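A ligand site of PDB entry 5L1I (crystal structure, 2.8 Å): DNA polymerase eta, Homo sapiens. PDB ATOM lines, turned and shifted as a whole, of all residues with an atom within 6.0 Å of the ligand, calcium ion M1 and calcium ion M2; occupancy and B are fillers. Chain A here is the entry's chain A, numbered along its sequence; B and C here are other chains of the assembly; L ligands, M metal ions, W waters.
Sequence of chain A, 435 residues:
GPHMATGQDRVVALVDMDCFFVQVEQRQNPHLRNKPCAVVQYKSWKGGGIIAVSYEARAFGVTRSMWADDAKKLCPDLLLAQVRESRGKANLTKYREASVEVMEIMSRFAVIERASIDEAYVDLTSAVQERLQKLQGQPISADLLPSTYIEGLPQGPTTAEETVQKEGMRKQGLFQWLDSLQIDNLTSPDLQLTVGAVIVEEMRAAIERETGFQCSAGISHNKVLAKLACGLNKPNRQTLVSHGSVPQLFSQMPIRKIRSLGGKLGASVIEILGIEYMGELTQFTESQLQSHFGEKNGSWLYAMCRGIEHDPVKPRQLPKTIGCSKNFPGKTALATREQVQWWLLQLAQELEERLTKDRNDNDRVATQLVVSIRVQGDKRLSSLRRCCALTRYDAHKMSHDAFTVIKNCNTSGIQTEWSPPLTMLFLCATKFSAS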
ATOM      1  N   ASP A  16     -17.076  19.413   3.390  1.00  0.00           N
ATOM      2  CA  ASP A  16     -15.865  20.217   3.469  1.00  0.00           C
ATOM      3  C   ASP A  16     -14.724  19.391   4.043  1.00  0.00           C
ATOM      4  O   ASP A  16     -14.894  18.728   5.070  1.00  0.00           O
ATOM      5  CB  ASP A  16     -16.103  21.398   4.408  1.00  0.00           C
ATOM      6  CG  ASP A  16     -14.802  22.037   4.878  1.00  0.00           C
ATOM      7  OD1 ASP A  16     -14.295  21.673   5.956  1.00  0.00           O
ATOM      8  OD2 ASP A  16     -14.246  22.861   4.123  1.00  0.00           O
ATOM      9  N   MET A  17     -13.555  19.484   3.456  1.00  0.00           N
ATOM     10  CA  MET A  17     -12.468  18.609   3.875  1.00  0.00           C
ATOM     11  C   MET A  17     -11.856  19.141   5.151  1.00  0.00           C
ATOM     12  O   MET A  17     -11.766  20.362   5.338  1.00  0.00           O
ATOM     13  CB  MET A  17     -11.396  18.512   2.782  1.00  0.00           C
ATOM     14  CG  MET A  17     -11.896  18.195   1.392  1.00  0.00           C
ATOM     15  SD  MET A  17     -12.986  16.770   1.328  1.00  0.00           S
ATOM     16  CE  MET A  17     -11.764  15.531   1.706  1.00  0.00           C
ATOM     17  N   ASP A  18     -11.407  18.210   6.011  1.00  0.00           N
ATOM     18  CA  ASP A  18     -10.719  18.576   7.248  1.00  0.00           C
ATOM     19  C   ASP A  18      -9.282  19.010   6.972  1.00  0.00           C
ATOM     20  O   ASP A  18      -8.566  18.309   6.259  1.00  0.00           O
ATOM     21  CB  ASP A  18     -10.728  17.418   8.234  1.00  0.00           C
ATOM     22  CG  ASP A  18     -12.119  16.939   8.516  1.00  0.00           C
ATOM     23  OD1 ASP A  18     -13.073  17.716   8.347  1.00  0.00           O
ATOM     24  OD2 ASP A  18     -12.254  15.755   8.868  1.00  0.00           O
ATOM     25  N   CYS A  19      -8.876  20.150   7.537  1.00  0.00           N
ATOM     26  CA  CYS A  19      -7.514  20.705   7.387  1.00  0.00           C
ATOM     27  C   CYS A  19      -6.911  20.336   6.023  1.00  0.00           C
ATOM     28  O   CYS A  19      -5.893  19.679   5.902  1.00  0.00           O
ATOM     29  CB  CYS A  19      -6.619  20.270   8.567  1.00  0.00           C
ATOM     30  SG  CYS A  19      -6.516  18.480   8.847  1.00  0.00           S
ATOM     31  N   PHE A  20      -7.607  20.751   4.985  1.00  0.00           N
ATOM     32  CA  PHE A  20      -7.384  20.187   3.669  1.00  0.00           C
ATOM     33  C   PHE A  20      -5.906  20.158   3.223  1.00  0.00           C
ATOM     34  O   PHE A  20      -5.333  19.094   3.009  1.00  0.00           O
ATOM     35  CB  PHE A  20      -8.233  20.880   2.615  1.00  0.00           C
ATOM     36  CG  PHE A  20      -8.193  20.210   1.280  1.00  0.00           C
ATOM     37  CD1 PHE A  20      -8.322  18.829   1.179  1.00  0.00           C
ATOM     38  CD2 PHE A  20      -8.027  20.940   0.129  1.00  0.00           C
ATOM     39  CE1 PHE A  20      -8.257  18.194  -0.053  1.00  0.00           C
ATOM     40  CE2 PHE A  20      -7.989  20.309  -1.117  1.00  0.00           C
ATOM     41  CZ  PHE A  20      -8.102  18.932  -1.203  1.00  0.00           C
ATOM     42  N   PHE A  21      -5.283  21.320   3.111  1.00  0.00           N
ATOM     43  CA  PHE A  21      -3.912  21.382   2.614  1.00  0.00           C
ATOM     44  C   PHE A  21      -2.967  20.538   3.444  1.00  0.00           C
ATOM     45  O   PHE A  21      -2.099  19.878   2.897  1.00  0.00           O
ATOM     46  CB  PHE A  21      -3.383  22.818   2.530  1.00  0.00           C
ATOM     47  CG  PHE A  21      -3.952  23.629   1.406  1.00  0.00           C
ATOM     48  CD1 PHE A  21      -5.150  23.316   0.776  1.00  0.00           C
ATOM     49  CD2 PHE A  21      -3.300  24.787   1.013  1.00  0.00           C
ATOM     50  CE1 PHE A  21      -5.662  24.113  -0.246  1.00  0.00           C
ATOM     51  CE2 PHE A  21      -3.807  25.598   0.007  1.00  0.00           C
ATOM     52  CZ  PHE A  21      -4.993  25.267  -0.621  1.00  0.00           C
ATOM     53  N   VAL A  22      -3.161  20.530   4.762  1.00  0.00           N
ATOM     54  CA  VAL A  22      -2.343  19.697   5.655  1.00  0.00           C
ATOM     55  C   VAL A  22      -2.547  18.219   5.333  1.00  0.00           C
ATOM     56  O   VAL A  22      -1.566  17.463   5.249  1.00  0.00           O
ATOM     57  CB  VAL A  22      -2.679  19.909   7.162  1.00  0.00           C
ATOM     58  CG1 VAL A  22      -1.758  19.048   8.016  1.00  0.00           C
ATOM     59  CG2 VAL A  22      -2.544  21.371   7.589  1.00  0.00           C
ATOM     60  N   GLN A  41       3.553  29.491   3.560  1.00  0.00           N
ATOM     61  CA  GLN A  41       3.777  30.221   2.334  1.00  0.00           C
ATOM     62  C   GLN A  41       4.871  31.224   2.491  1.00  0.00           C
ATOM     63  O   GLN A  41       4.745  32.116   3.268  1.00  0.00           O
ATOM     64  CB  GLN A  41       2.510  31.015   2.061  1.00  0.00           C
ATOM     65  CG  GLN A  41       2.009  31.050   0.639  1.00  0.00           C
ATOM     66  CD  GLN A  41       0.678  31.739   0.534  1.00  0.00           C
ATOM     67  OE1 GLN A  41      -0.157  31.351  -0.246  1.00  0.00           O
ATOM     68  NE2 GLN A  41       0.478  32.759   1.326  1.00  0.00           N
ATOM     69  N   ILE A  51      -1.203  28.967   6.334  1.00  0.00           N
ATOM     70  CA  ILE A  51      -2.502  28.888   5.649  1.00  0.00           C
ATOM     71  C   ILE A  51      -3.359  27.668   5.997  1.00  0.00           C
ATOM     72  O   ILE A  51      -4.528  27.639   5.624  1.00  0.00           O
ATOM     73  CB  ILE A  51      -2.354  29.021   4.120  1.00  0.00           C
ATOM     74  CG1 ILE A  51      -1.676  27.800   3.496  1.00  0.00           C
ATOM     75  CG2 ILE A  51      -1.607  30.318   3.801  1.00  0.00           C
ATOM     76  CD1 ILE A  51      -1.445  27.937   1.992  1.00  0.00           C
ATOM     77  N   ALA A  52      -2.803  26.685   6.703  1.00  0.00           N
ATOM     78  CA  ALA A  52      -3.575  25.525   7.148  1.00  0.00           C
ATOM     79  C   ALA A  52      -2.913  24.899   8.369  1.00  0.00           C
ATOM     80  O   ALA A  52      -1.678  24.941   8.477  1.00  0.00           O
ATOM     81  CB  ALA A  52      -3.688  24.532   6.011  1.00  0.00           C
ATOM     82  N   VAL A  53      -3.719  24.340   9.285  1.00  0.00           N
ATOM     83  CA  VAL A  53      -3.237  23.881  10.613  1.00  0.00           C
ATOM     84  C   VAL A  53      -3.876  22.552  10.968  1.00  0.00           C
ATOM     85  O   VAL A  53      -5.089  22.432  10.915  1.00  0.00           O
ATOM     86  CB  VAL A  53      -3.578  24.894  11.727  1.00  0.00           C
ATOM     87  CG1 VAL A  53      -2.765  24.600  12.987  1.00  0.00           C
ATOM     88  CG2 VAL A  53      -3.300  26.311  11.290  1.00  0.00           C
ATOM     89  N   TYR A  55      -5.233  19.419  13.398  1.00  0.00           N
ATOM     90  CA  TYR A  55      -6.044  19.490  14.626  1.00  0.00           C
ATOM     91  C   TYR A  55      -5.215  19.328  15.913  1.00  0.00           C
ATOM     92  O   TYR A  55      -5.520  19.935  16.942  1.00  0.00           O
ATOM     93  CB  TYR A  55      -7.262  18.537  14.575  1.00  0.00           C
ATOM     94  CG  TYR A  55      -8.363  19.141  13.760  1.00  0.00           C
ATOM     95  CD1 TYR A  55      -8.322  19.106  12.364  1.00  0.00           C
ATOM     96  CD2 TYR A  55      -9.409  19.849  14.378  1.00  0.00           C
ATOM     97  CE1 TYR A  55      -9.319  19.702  11.603  1.00  0.00           C
ATOM     98  CE2 TYR A  55     -10.404  20.457  13.624  1.00  0.00           C
ATOM     99  CZ  TYR A  55     -10.363  20.381  12.227  1.00  0.00           C
ATOM    100  OH  TYR A  55     -11.346  20.994  11.445  1.00  0.00           O
ATOM    101  N   ARG A  58      -3.768  22.724  16.417  1.00  0.00           N
ATOM    102  CA  ARG A  58      -4.806  23.636  16.927  1.00  0.00           C
ATOM    103  C   ARG A  58      -4.934  23.557  18.457  1.00  0.00           C
ATOM    104  O   ARG A  58      -5.130  24.578  19.107  1.00  0.00           O
ATOM    105  CB  ARG A  58      -6.160  23.379  16.250  1.00  0.00           C
ATOM    106  CG  ARG A  58      -6.217  23.857  14.804  1.00  0.00           C
ATOM    107  CD  ARG A  58      -7.529  23.499  14.116  1.00  0.00           C
ATOM    108  NE  ARG A  58      -7.364  23.291  12.666  1.00  0.00           N
ATOM    109  CZ  ARG A  58      -8.350  23.272  11.761  1.00  0.00           C
ATOM    110  NH1 ARG A  58      -9.615  23.445  12.098  1.00  0.00           N
ATOM    111  NH2 ARG A  58      -8.029  23.076  10.483  1.00  0.00           N
ATOM    112  N   ARG A  64      -4.427  30.043  11.378  1.00  0.00           N
ATOM    113  CA  ARG A  64      -4.174  30.656  10.074  1.00  0.00           C
ATOM    114  C   ARG A  64      -3.810  32.151  10.250  1.00  0.00           C
ATOM    115  O   ARG A  64      -4.125  32.736  11.277  1.00  0.00           O
ATOM    116  CB  ARG A  64      -5.431  30.444   9.222  1.00  0.00           C
ATOM    117  CG  ARG A  64      -5.427  30.977   7.806  1.00  0.00           C
ATOM    118  CD  ARG A  64      -6.323  30.169   6.871  1.00  0.00           C
ATOM    119  NE  ARG A  64      -7.632  29.850   7.433  1.00  0.00           N
ATOM    120  CZ  ARG A  64      -8.305  28.702   7.254  1.00  0.00           C
ATOM    121  NH1 ARG A  64      -9.482  28.527   7.843  1.00  0.00           N
ATOM    122  NH2 ARG A  64      -7.827  27.700   6.503  1.00  0.00           N
ATOM    123  N   SER A 116     -15.746  25.917  -3.096  1.00  0.00           N
ATOM    124  CA  SER A 116     -14.383  26.331  -2.799  1.00  0.00           C
ATOM    125  C   SER A 116     -13.494  25.188  -3.210  1.00  0.00           C
ATOM    126  O   SER A 116     -13.998  24.142  -3.624  1.00  0.00           O
ATOM    127  CB  SER A 116     -14.189  26.590  -1.289  1.00  0.00           C
ATOM    128  OG  SER A 116     -13.912  25.385  -0.520  1.00  0.00           O
ATOM    129  N   ILE A 117     -12.175  25.324  -3.035  1.00  0.00           N
ATOM    130  CA  ILE A 117     -11.253  24.250  -3.378  1.00  0.00           C
ATOM    131  C   ILE A 117     -11.496  22.974  -2.585  1.00  0.00           C
ATOM    132  O   ILE A 117     -11.300  21.894  -3.123  1.00  0.00           O
ATOM    133  CB  ILE A 117      -9.772  24.666  -3.229  1.00  0.00           C
ATOM    134  CG1 ILE A 117      -8.860  23.678  -3.982  1.00  0.00           C
ATOM    135  CG2 ILE A 117      -9.361  24.771  -1.778  1.00  0.00           C
ATOM    136  CD1 ILE A 117      -7.413  24.143  -4.018  1.00  0.00           C
ATOM    137  N   ASP A 118     -11.939  23.090  -1.332  1.00  0.00           N
ATOM    138  CA  ASP A 118     -12.199  21.888  -0.520  1.00  0.00           C
ATOM    139  C   ASP A 118     -13.639  21.699  -0.109  1.00  0.00           C
ATOM    140  O   ASP A 118     -13.861  20.899   0.786  1.00  0.00           O
ATOM    141  CB  ASP A 118     -11.271  21.841   0.726  1.00  0.00           C
ATOM    142  CG  ASP A 118     -11.814  22.634   1.878  1.00  0.00           C
ATOM    143  OD1 ASP A 118     -12.288  23.764   1.629  1.00  0.00           O
ATOM    144  OD2 ASP A 118     -11.808  22.117   3.025  1.00  0.00           O
ATOM    145  N   GLU A 119     -14.606  22.381  -0.717  1.00  0.00           N
ATOM    146  CA  GLU A 119     -16.034  22.149  -0.365  1.00  0.00           C
ATOM    147  C   GLU A 119     -17.051  22.294  -1.496  1.00  0.00           C
ATOM    148  O   GLU A 119     -16.992  23.219  -2.301  1.00  0.00           O
ATOM    149  CB  GLU A 119     -16.455  22.982   0.865  1.00  0.00           C
ATOM    150  CG  GLU A 119     -16.923  24.390   0.567  1.00  0.00           C
ATOM    151  CD  GLU A 119     -17.057  25.245   1.802  1.00  0.00           C
ATOM    152  OE1 GLU A 119     -18.121  25.890   1.941  1.00  0.00           O
ATOM    153  OE2 GLU A 119     -16.132  25.288   2.657  1.00  0.00           O
ATOM    154  N   LYS A 227     -24.283  24.167   5.584  1.00  0.00           N
ATOM    155  CA  LYS A 227     -23.026  24.844   5.962  1.00  0.00           C
ATOM    156  C   LYS A 227     -22.830  24.922   7.493  1.00  0.00           C
ATOM    157  O   LYS A 227     -21.882  24.362   8.057  1.00  0.00           O
ATOM    158  CB  LYS A 227     -23.001  26.230   5.315  1.00  0.00           C
ATOM    159  CG  LYS A 227     -21.843  27.150   5.677  1.00  0.00           C
ATOM    160  CD  LYS A 227     -20.526  26.670   5.126  1.00  0.00           C
ATOM    161  CE  LYS A 227     -19.485  27.782   5.144  1.00  0.00           C
ATOM    162  NZ  LYS A 227     -18.132  27.190   4.924  1.00  0.00           N
ATOM    163  N   LYS A 234     -16.790  18.797  13.950  1.00  0.00           N
ATOM    164  CA  LYS A 234     -15.565  18.581  13.191  1.00  0.00           C
ATOM    165  C   LYS A 234     -14.578  18.048  14.202  1.00  0.00           C
ATOM    166  O   LYS A 234     -14.759  18.318  15.370  1.00  0.00           O
ATOM    167  CB  LYS A 234     -15.057  19.890  12.615  1.00  0.00           C
ATOM    168  CG  LYS A 234     -15.517  20.149  11.209  1.00  0.00           C
ATOM    169  CD  LYS A 234     -14.673  21.228  10.542  1.00  0.00           C
ATOM    170  CE  LYS A 234     -14.865  21.268   9.034  1.00  0.00           C
ATOM    171  NZ  LYS A 234     -13.994  20.275   8.374  1.00  0.00           N
ATOM    172  P    DT B   8     -16.194  30.601   5.440  1.00  0.00           P
ATOM    173  OP1  DT B   8     -17.043  30.005   6.499  1.00  0.00           O
ATOM    174  OP2  DT B   8     -14.959  31.362   5.793  1.00  0.00           O
ATOM    175  O5'  DT B   8     -15.770  29.455   4.429  1.00  0.00           O
ATOM    176  C5'  DT B   8     -15.524  29.774   3.048  1.00  0.00           C
ATOM    177  C4'  DT B   8     -14.044  29.814   2.736  1.00  0.00           C
ATOM    178  O4'  DT B   8     -13.506  31.130   2.516  1.00  0.00           O
ATOM    179  C3'  DT B   8     -13.075  29.138   3.712  1.00  0.00           C
ATOM    180  O3'  DT B   8     -12.666  27.860   3.249  1.00  0.00           O
ATOM    181  C2'  DT B   8     -11.830  30.025   3.682  1.00  0.00           C
ATOM    182  C1'  DT B   8     -12.097  30.974   2.527  1.00  0.00           C
ATOM    183  N1   DT B   8     -11.484  32.294   2.673  1.00  0.00           N
ATOM    184  C2   DT B   8     -10.519  32.668   1.770  1.00  0.00           C
ATOM    185  O2   DT B   8     -10.150  31.957   0.854  1.00  0.00           O
ATOM    186  N3   DT B   8      -9.996  33.920   1.985  1.00  0.00           N
ATOM    187  C4   DT B   8     -10.339  34.806   2.990  1.00  0.00           C
ATOM    188  O4   DT B   8      -9.774  35.900   3.067  1.00  0.00           O
ATOM    189  C5   DT B   8     -11.361  34.346   3.901  1.00  0.00           C
ATOM    190  C7   DT B   8     -11.787  35.229   5.033  1.00  0.00           C
ATOM    191  C6   DT B   8     -11.881  33.127   3.699  1.00  0.00           C
ATOM    192  P    DC B   9     -12.649  27.554   1.700  1.00  0.00           P
ATOM    193  OP1  DC B   9     -13.501  28.547   0.996  1.00  0.00           O
ATOM    194  OP2  DC B   9     -12.931  26.104   1.550  1.00  0.00           O
ATOM    195  O5'  DC B   9     -11.159  27.923   1.238  1.00  0.00           O
ATOM    196  C5'  DC B   9     -10.542  27.146   0.176  1.00  0.00           C
ATOM    197  C4'  DC B   9      -9.794  27.964  -0.849  1.00  0.00           C
ATOM    198  O4'  DC B   9     -10.455  27.847  -2.136  1.00  0.00           O
ATOM    199  C3'  DC B   9      -9.682  29.472  -0.633  1.00  0.00           C
ATOM    200  O3'  DC B   9      -8.624  29.785   0.262  1.00  0.00           O
ATOM    201  C2'  DC B   9      -9.385  29.955  -2.039  1.00  0.00           C
ATOM    202  C1'  DC B   9     -10.263  29.041  -2.901  1.00  0.00           C
ATOM    203  N1   DC B   9     -11.602  29.547  -3.284  1.00  0.00           N
ATOM    204  C2   DC B   9     -12.263  28.922  -4.346  1.00  0.00           C
ATOM    205  O2   DC B   9     -11.705  27.988  -4.957  1.00  0.00           O
ATOM    206  N3   DC B   9     -13.510  29.354  -4.687  1.00  0.00           N
ATOM    207  C4   DC B   9     -14.070  30.351  -4.016  1.00  0.00           C
ATOM    208  N4   DC B   9     -15.295  30.748  -4.388  1.00  0.00           N
ATOM    209  C5   DC B   9     -13.423  31.000  -2.932  1.00  0.00           C
ATOM    210  C6   DC B   9     -12.198  30.565  -2.594  1.00  0.00           C
ATOM    211  P    DT C   3      -0.221  41.997   8.445  1.00  0.00           P
ATOM    212  OP1  DT C   3      -0.768  43.292   7.942  1.00  0.00           O
ATOM    213  OP2  DT C   3      -0.480  41.588   9.842  1.00  0.00           O
ATOM    214  O5'  DT C   3      -0.747  40.902   7.422  1.00  0.00           O
ATOM    215  C5'  DT C   3      -0.817  39.507   7.760  1.00  0.00           C
ATOM    216  C4'  DT C   3      -0.009  38.687   6.785  1.00  0.00           C
ATOM    217  O4'  DT C   3      -0.327  37.292   6.959  1.00  0.00           O
ATOM    218  C3'  DT C   3      -0.233  39.016   5.303  1.00  0.00           C
ATOM    219  O3'  DT C   3       0.997  39.297   4.604  1.00  0.00           O
ATOM    220  C2'  DT C   3      -0.937  37.802   4.728  1.00  0.00           C
ATOM    221  C1'  DT C   3      -0.753  36.693   5.755  1.00  0.00           C
ATOM    222  N1   DT C   3      -2.000  35.951   6.032  1.00  0.00           N
ATOM    223  C2   DT C   3      -2.039  34.573   5.856  1.00  0.00           C
ATOM    224  O2   DT C   3      -1.067  33.915   5.512  1.00  0.00           O
ATOM    225  N3   DT C   3      -3.249  33.999   6.132  1.00  0.00           N
ATOM    226  C4   DT C   3      -4.404  34.643   6.553  1.00  0.00           C
ATOM    227  O4   DT C   3      -5.423  33.983   6.764  1.00  0.00           O
ATOM    228  C5   DT C   3      -4.293  36.084   6.700  1.00  0.00           C
ATOM    229  C7   DT C   3      -5.500  36.861   7.138  1.00  0.00           C
ATOM    230  C6   DT C   3      -3.110  36.648   6.435  1.00  0.00           C
ATOM    231  P   6OG C   4       0.984  40.027   3.156  1.00  0.00           P
ATOM    232  OP1 6OG C   4       2.365  40.546   2.878  1.00  0.00           O
ATOM    233  OP2 6OG C   4      -0.204  40.940   3.119  1.00  0.00           O
ATOM    234  O5' 6OG C   4       0.714  38.813   2.127  1.00  0.00           O
ATOM    235  N9  6OG C   4      -2.355  36.101   1.446  1.00  0.00           N
ATOM    236  C4  6OG C   4      -3.100  35.035   1.641  1.00  0.00           C
ATOM    237  N3  6OG C   4      -2.927  33.728   1.353  1.00  0.00           N
ATOM    238  C2  6OG C   4      -3.875  32.818   1.709  1.00  0.00           C
ATOM    239  N2  6OG C   4      -3.653  31.528   1.379  1.00  0.00           N
ATOM    240  N1  6OG C   4      -5.018  33.140   2.348  1.00  0.00           N
ATOM    241  C6  6OG C   4      -5.298  34.407   2.694  1.00  0.00           C
ATOM    242  O6  6OG C   4      -6.490  34.653   3.336  1.00  0.00           O
ATOM    243  C5  6OG C   4      -4.322  35.453   2.337  1.00  0.00           C
ATOM    244  N7  6OG C   4      -4.220  36.774   2.505  1.00  0.00           N
ATOM    245  C8  6OG C   4      -3.027  37.165   1.955  1.00  0.00           C
ATOM    246  C2' 6OG C   4      -0.793  37.246  -0.191  1.00  0.00           C
ATOM    247  C5' 6OG C   4       1.726  37.839   1.870  1.00  0.00           C
ATOM    248  C4' 6OG C   4       1.204  36.706   1.006  1.00  0.00           C
ATOM    249  O4' 6OG C   4       0.096  36.057   1.657  1.00  0.00           O
ATOM    250  C1' 6OG C   4      -1.026  36.066   0.759  1.00  0.00           C
ATOM    251  C3' 6OG C   4       0.711  37.208  -0.351  1.00  0.00           C
ATOM    252  O3' 6OG C   4       1.149  36.275  -1.333  1.00  0.00           O
ATOM    253  C   6OG C   4      -6.790  35.791   4.154  1.00  0.00           C
ATOM    254  P    DA C   5       0.714  36.440  -2.855  1.00  0.00           P
ATOM    255  OP1  DA C   5       1.849  36.031  -3.707  1.00  0.00           O
ATOM    256  OP2  DA C   5       0.135  37.775  -3.053  1.00  0.00           O
ATOM    257  O5'  DA C   5      -0.476  35.391  -2.988  1.00  0.00           O
ATOM    258  C5'  DA C   5      -0.215  33.969  -3.039  1.00  0.00           C
ATOM    259  C4'  DA C   5      -1.489  33.207  -3.324  1.00  0.00           C
ATOM    260  O4'  DA C   5      -2.480  33.465  -2.288  1.00  0.00           O
ATOM    261  C3'  DA C   5      -2.150  33.583  -4.657  1.00  0.00           C
ATOM    262  O3'  DA C   5      -2.389  32.379  -5.416  1.00  0.00           O
ATOM    263  C2'  DA C   5      -3.345  34.428  -4.239  1.00  0.00           C
ATOM    264  C1'  DA C   5      -3.711  33.833  -2.890  1.00  0.00           C
ATOM    265  N9   DA C   5      -4.426  34.732  -1.977  1.00  0.00           N
ATOM    266  C8   DA C   5      -4.118  36.027  -1.646  1.00  0.00           C
ATOM    267  N7   DA C   5      -4.964  36.568  -0.805  1.00  0.00           N
ATOM    268  C5   DA C   5      -5.903  35.569  -0.581  1.00  0.00           C
ATOM    269  C6   DA C   5      -7.069  35.519   0.201  1.00  0.00           C
ATOM    270  N6   DA C   5      -7.504  36.537   0.955  1.00  0.00           N
ATOM    271  N1   DA C   5      -7.789  34.381   0.189  1.00  0.00           N
ATOM    272  C2   DA C   5      -7.360  33.364  -0.553  1.00  0.00           C
ATOM    273  N3   DA C   5      -6.286  33.282  -1.336  1.00  0.00           N
ATOM    274  C4   DA C   5      -5.588  34.433  -1.298  1.00  0.00           C
HETATM  275  N1  LIG L   1      -7.103  28.300   2.672  1.00  0.00           N
HETATM  276  C1  LIG L   1      -6.181  29.328   2.404  1.00  0.00           C
HETATM  277  N2  LIG L   1      -6.374  30.589   2.873  1.00  0.00           N
HETATM  278  C2  LIG L   1      -7.477  30.878   3.625  1.00  0.00           C
HETATM  279  C3  LIG L   1      -8.372  29.867   3.913  1.00  0.00           C
HETATM  280  C4  LIG L   1      -8.173  28.582   3.426  1.00  0.00           C
HETATM  281  O1  LIG L   1      -5.185  29.072   1.713  1.00  0.00           O
HETATM  282  N3  LIG L   1      -7.749  32.109   4.140  1.00  0.00           N
HETATM  283  C5  LIG L   1      -6.869  26.941   2.159  1.00  0.00           C
HETATM  284  C6  LIG L   1      -6.088  26.117   3.160  1.00  0.00           C
HETATM  285  C7  LIG L   1      -7.106  25.165   3.736  1.00  0.00           C
HETATM  286  C8  LIG L   1      -8.166  25.052   2.673  1.00  0.00           C
HETATM  287  O2  LIG L   1      -8.110  26.271   1.948  1.00  0.00           O
HETATM  288  O3  LIG L   1      -6.506  23.918   4.003  1.00  0.00           O
HETATM  289  C9  LIG L   1      -9.603  24.919   3.156  1.00  0.00           C
HETATM  290  O4  LIG L   1      -9.849  25.930   4.119  1.00  0.00           O
HETATM  291  P1  LIG L   1     -10.988  25.821   5.243  1.00  0.00           P
HETATM  292  O5  LIG L   1     -11.267  27.251   5.635  1.00  0.00           O
HETATM  293  O6  LIG L   1     -11.993  24.810   4.765  1.00  0.00           O
HETATM  294  O7  LIG L   1     -10.263  25.151   6.519  1.00  0.00           O
HETATM  295  P2  LIG L   1      -9.341  23.831   6.520  1.00  0.00           P
HETATM  296  O8  LIG L   1      -7.868  24.211   6.549  1.00  0.00           O
HETATM  297  O9  LIG L   1      -9.866  22.858   5.541  1.00  0.00           O
HETATM  298  O10 LIG L   1      -9.681  23.229   7.970  1.00  0.00           O
HETATM  299  P3  LIG L   1     -11.170  22.996   8.540  1.00  0.00           P
HETATM  300  O11 LIG L   1     -11.297  23.976   9.687  1.00  0.00           O
HETATM  301  O12 LIG L   1     -12.078  23.278   7.370  1.00  0.00           O
HETATM  302  O13 LIG L   1     -11.092  21.555   9.024  1.00  0.00           O
HETATM  303 CA    CA M   1     -12.014  22.631   5.260  1.00  0.00          CA
HETATM  304 CA    CA M   2     -13.881  24.946   3.207  1.00  0.00          CA
HETATM  305  O   HOH W   1     -14.433  24.987   8.036  1.00  0.00           O
HETATM  306  O   HOH W   2     -10.709  26.463  10.017  1.00  0.00           O
HETATM  307  O   HOH W   3     -12.997  27.144   8.516  1.00  0.00           O
HETATM  308  O   HOH W   4     -14.636  25.896   5.250  1.00  0.00           O
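Calcium ion M1 is bound by O9 of the ligand, O12 of the ligand, O6 of the ligand, O of Met 17, OD2 of Asp 118, OD2 of Asp 16 and OD1 of Asp 16.
Calcium ion M1 has seven donor atoms within binding distance.
OH of Tyr 55 lies within hydrogen-bond range of O13 of the ligand, 2.5 Å away.
An oxygen (O5) of the ligand lies close to O3' of DT 8 of chain B, at 2.8 Å.
O6 of 6OG 4 of chain C lies within hydrogen-bond range of N3 of the ligand (3.0 Å).
The guanidinium group (NH1) of Arg 58 lies within salt-bridge range of an oxygen (O11) of the ligand.
The backbone NH of Phe 21 sits at hydrogen-bond distance from an oxygen (O3) of the ligand (3.0 Å).
An oxygen (O13) of the ligand sits at hydrogen-bond distance from the backbone NH of Cys 19, at 3.0 Å.
NH1 of Arg 64 is in salt-bridge range of O5 of the ligand.
The backbone NH of Phe 20 is in hydrogen-bond range of an oxygen (O3) of the ligand, 3.5 Å away.
The side-chain amino group (NZ) of Lys 234 lies within salt-bridge range of an oxygen (O13) of the ligand (3.2 Å).
OP2 of DC 9 of chain B lies close to the side-chain hydroxyl (OG) of Ser 116 (2.4 Å).
The side-chain hydroxyl of Ser 116 is in hydrogen-bond range of the backbone NH of Glu 119, 3.1 Å away.
The side-chain carboxylate (OE1) of Glu 119 lies within salt-bridge range of the side-chain amino group (NZ) of Lys 227 (3.3 Å).
OH of Tyr 55 sits at hydrogen-bond distance from NH1 of Arg 58, 3.1 Å away.
OP1 of DT 8 of chain B is in salt-bridge range of the side-chain amino group (NZ) of Lys 227 (3.4 Å).
O4' of 6OG 4 of chain C sits at hydrogen-bond distance from NE2 of Gln 41 (3.3 Å).
The guanidinium group of Arg 58 is in hydrogen-bond range of the backbone carbonyl oxygen of Val 53.
The backbone carbonyl oxygen of Ile 51 lies close to the guanidinium group of Arg 64 (3.4 Å).
Water W2 bridges an oxygen (O11) of the ligand and the guanidinium group (NH1) of Arg 64.
Within 4 Å of calcium ion M1: Asp 16, Met 17 and Asp 118.
Residues that only touch the ligand: Asp 18, Ile 51, Ala 52 and DT 3 of chain C.
Hydrophobic or aromatic side chains that line the ligand: Phe 20, Phe 21, Ile 51, Ala 52 and Tyr 55.
Within 4 Å of the ligand: Asp 16, Met 17, Asp 18, Cys 19, Phe 20, Phe 21, Ile 51, Ala 52, Tyr 55, Arg 58, Arg 64, Asp 118, Lys 234, DT 8 of chain B, DC 9 of chain B, DT 3 of chain C and 6OG 4 of chain C.
Along chain A the residues within 4 Å of the ligand span positions 16 to 234.
OP2 of DC 9 of chain B is bound to calcium ion M2.
OD2 of Asp 16 binds calcium ion M2 (2.3 Å).
OE2 of Glu 119 binds calcium ion M2 (2.3 Å).
Calcium ion M2 is bound by water W4 (2.4 Å).
Calcium ion M2 is bound by an oxygen (O6) of the ligand (2.5 Å).
OD1 of Asp 118 is bound to calcium ion M2 (2.5 Å).
Calcium ion M2 has six donor atoms within binding distance.
Merely in contact with calcium ion M2: DT 8 of chain B and Ser 116.
Within 4 Å of calcium ion M2: Asp 16, Ser 116, Asp 118, Glu 119, DT 8 of chain B and DC 9 of chain B.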
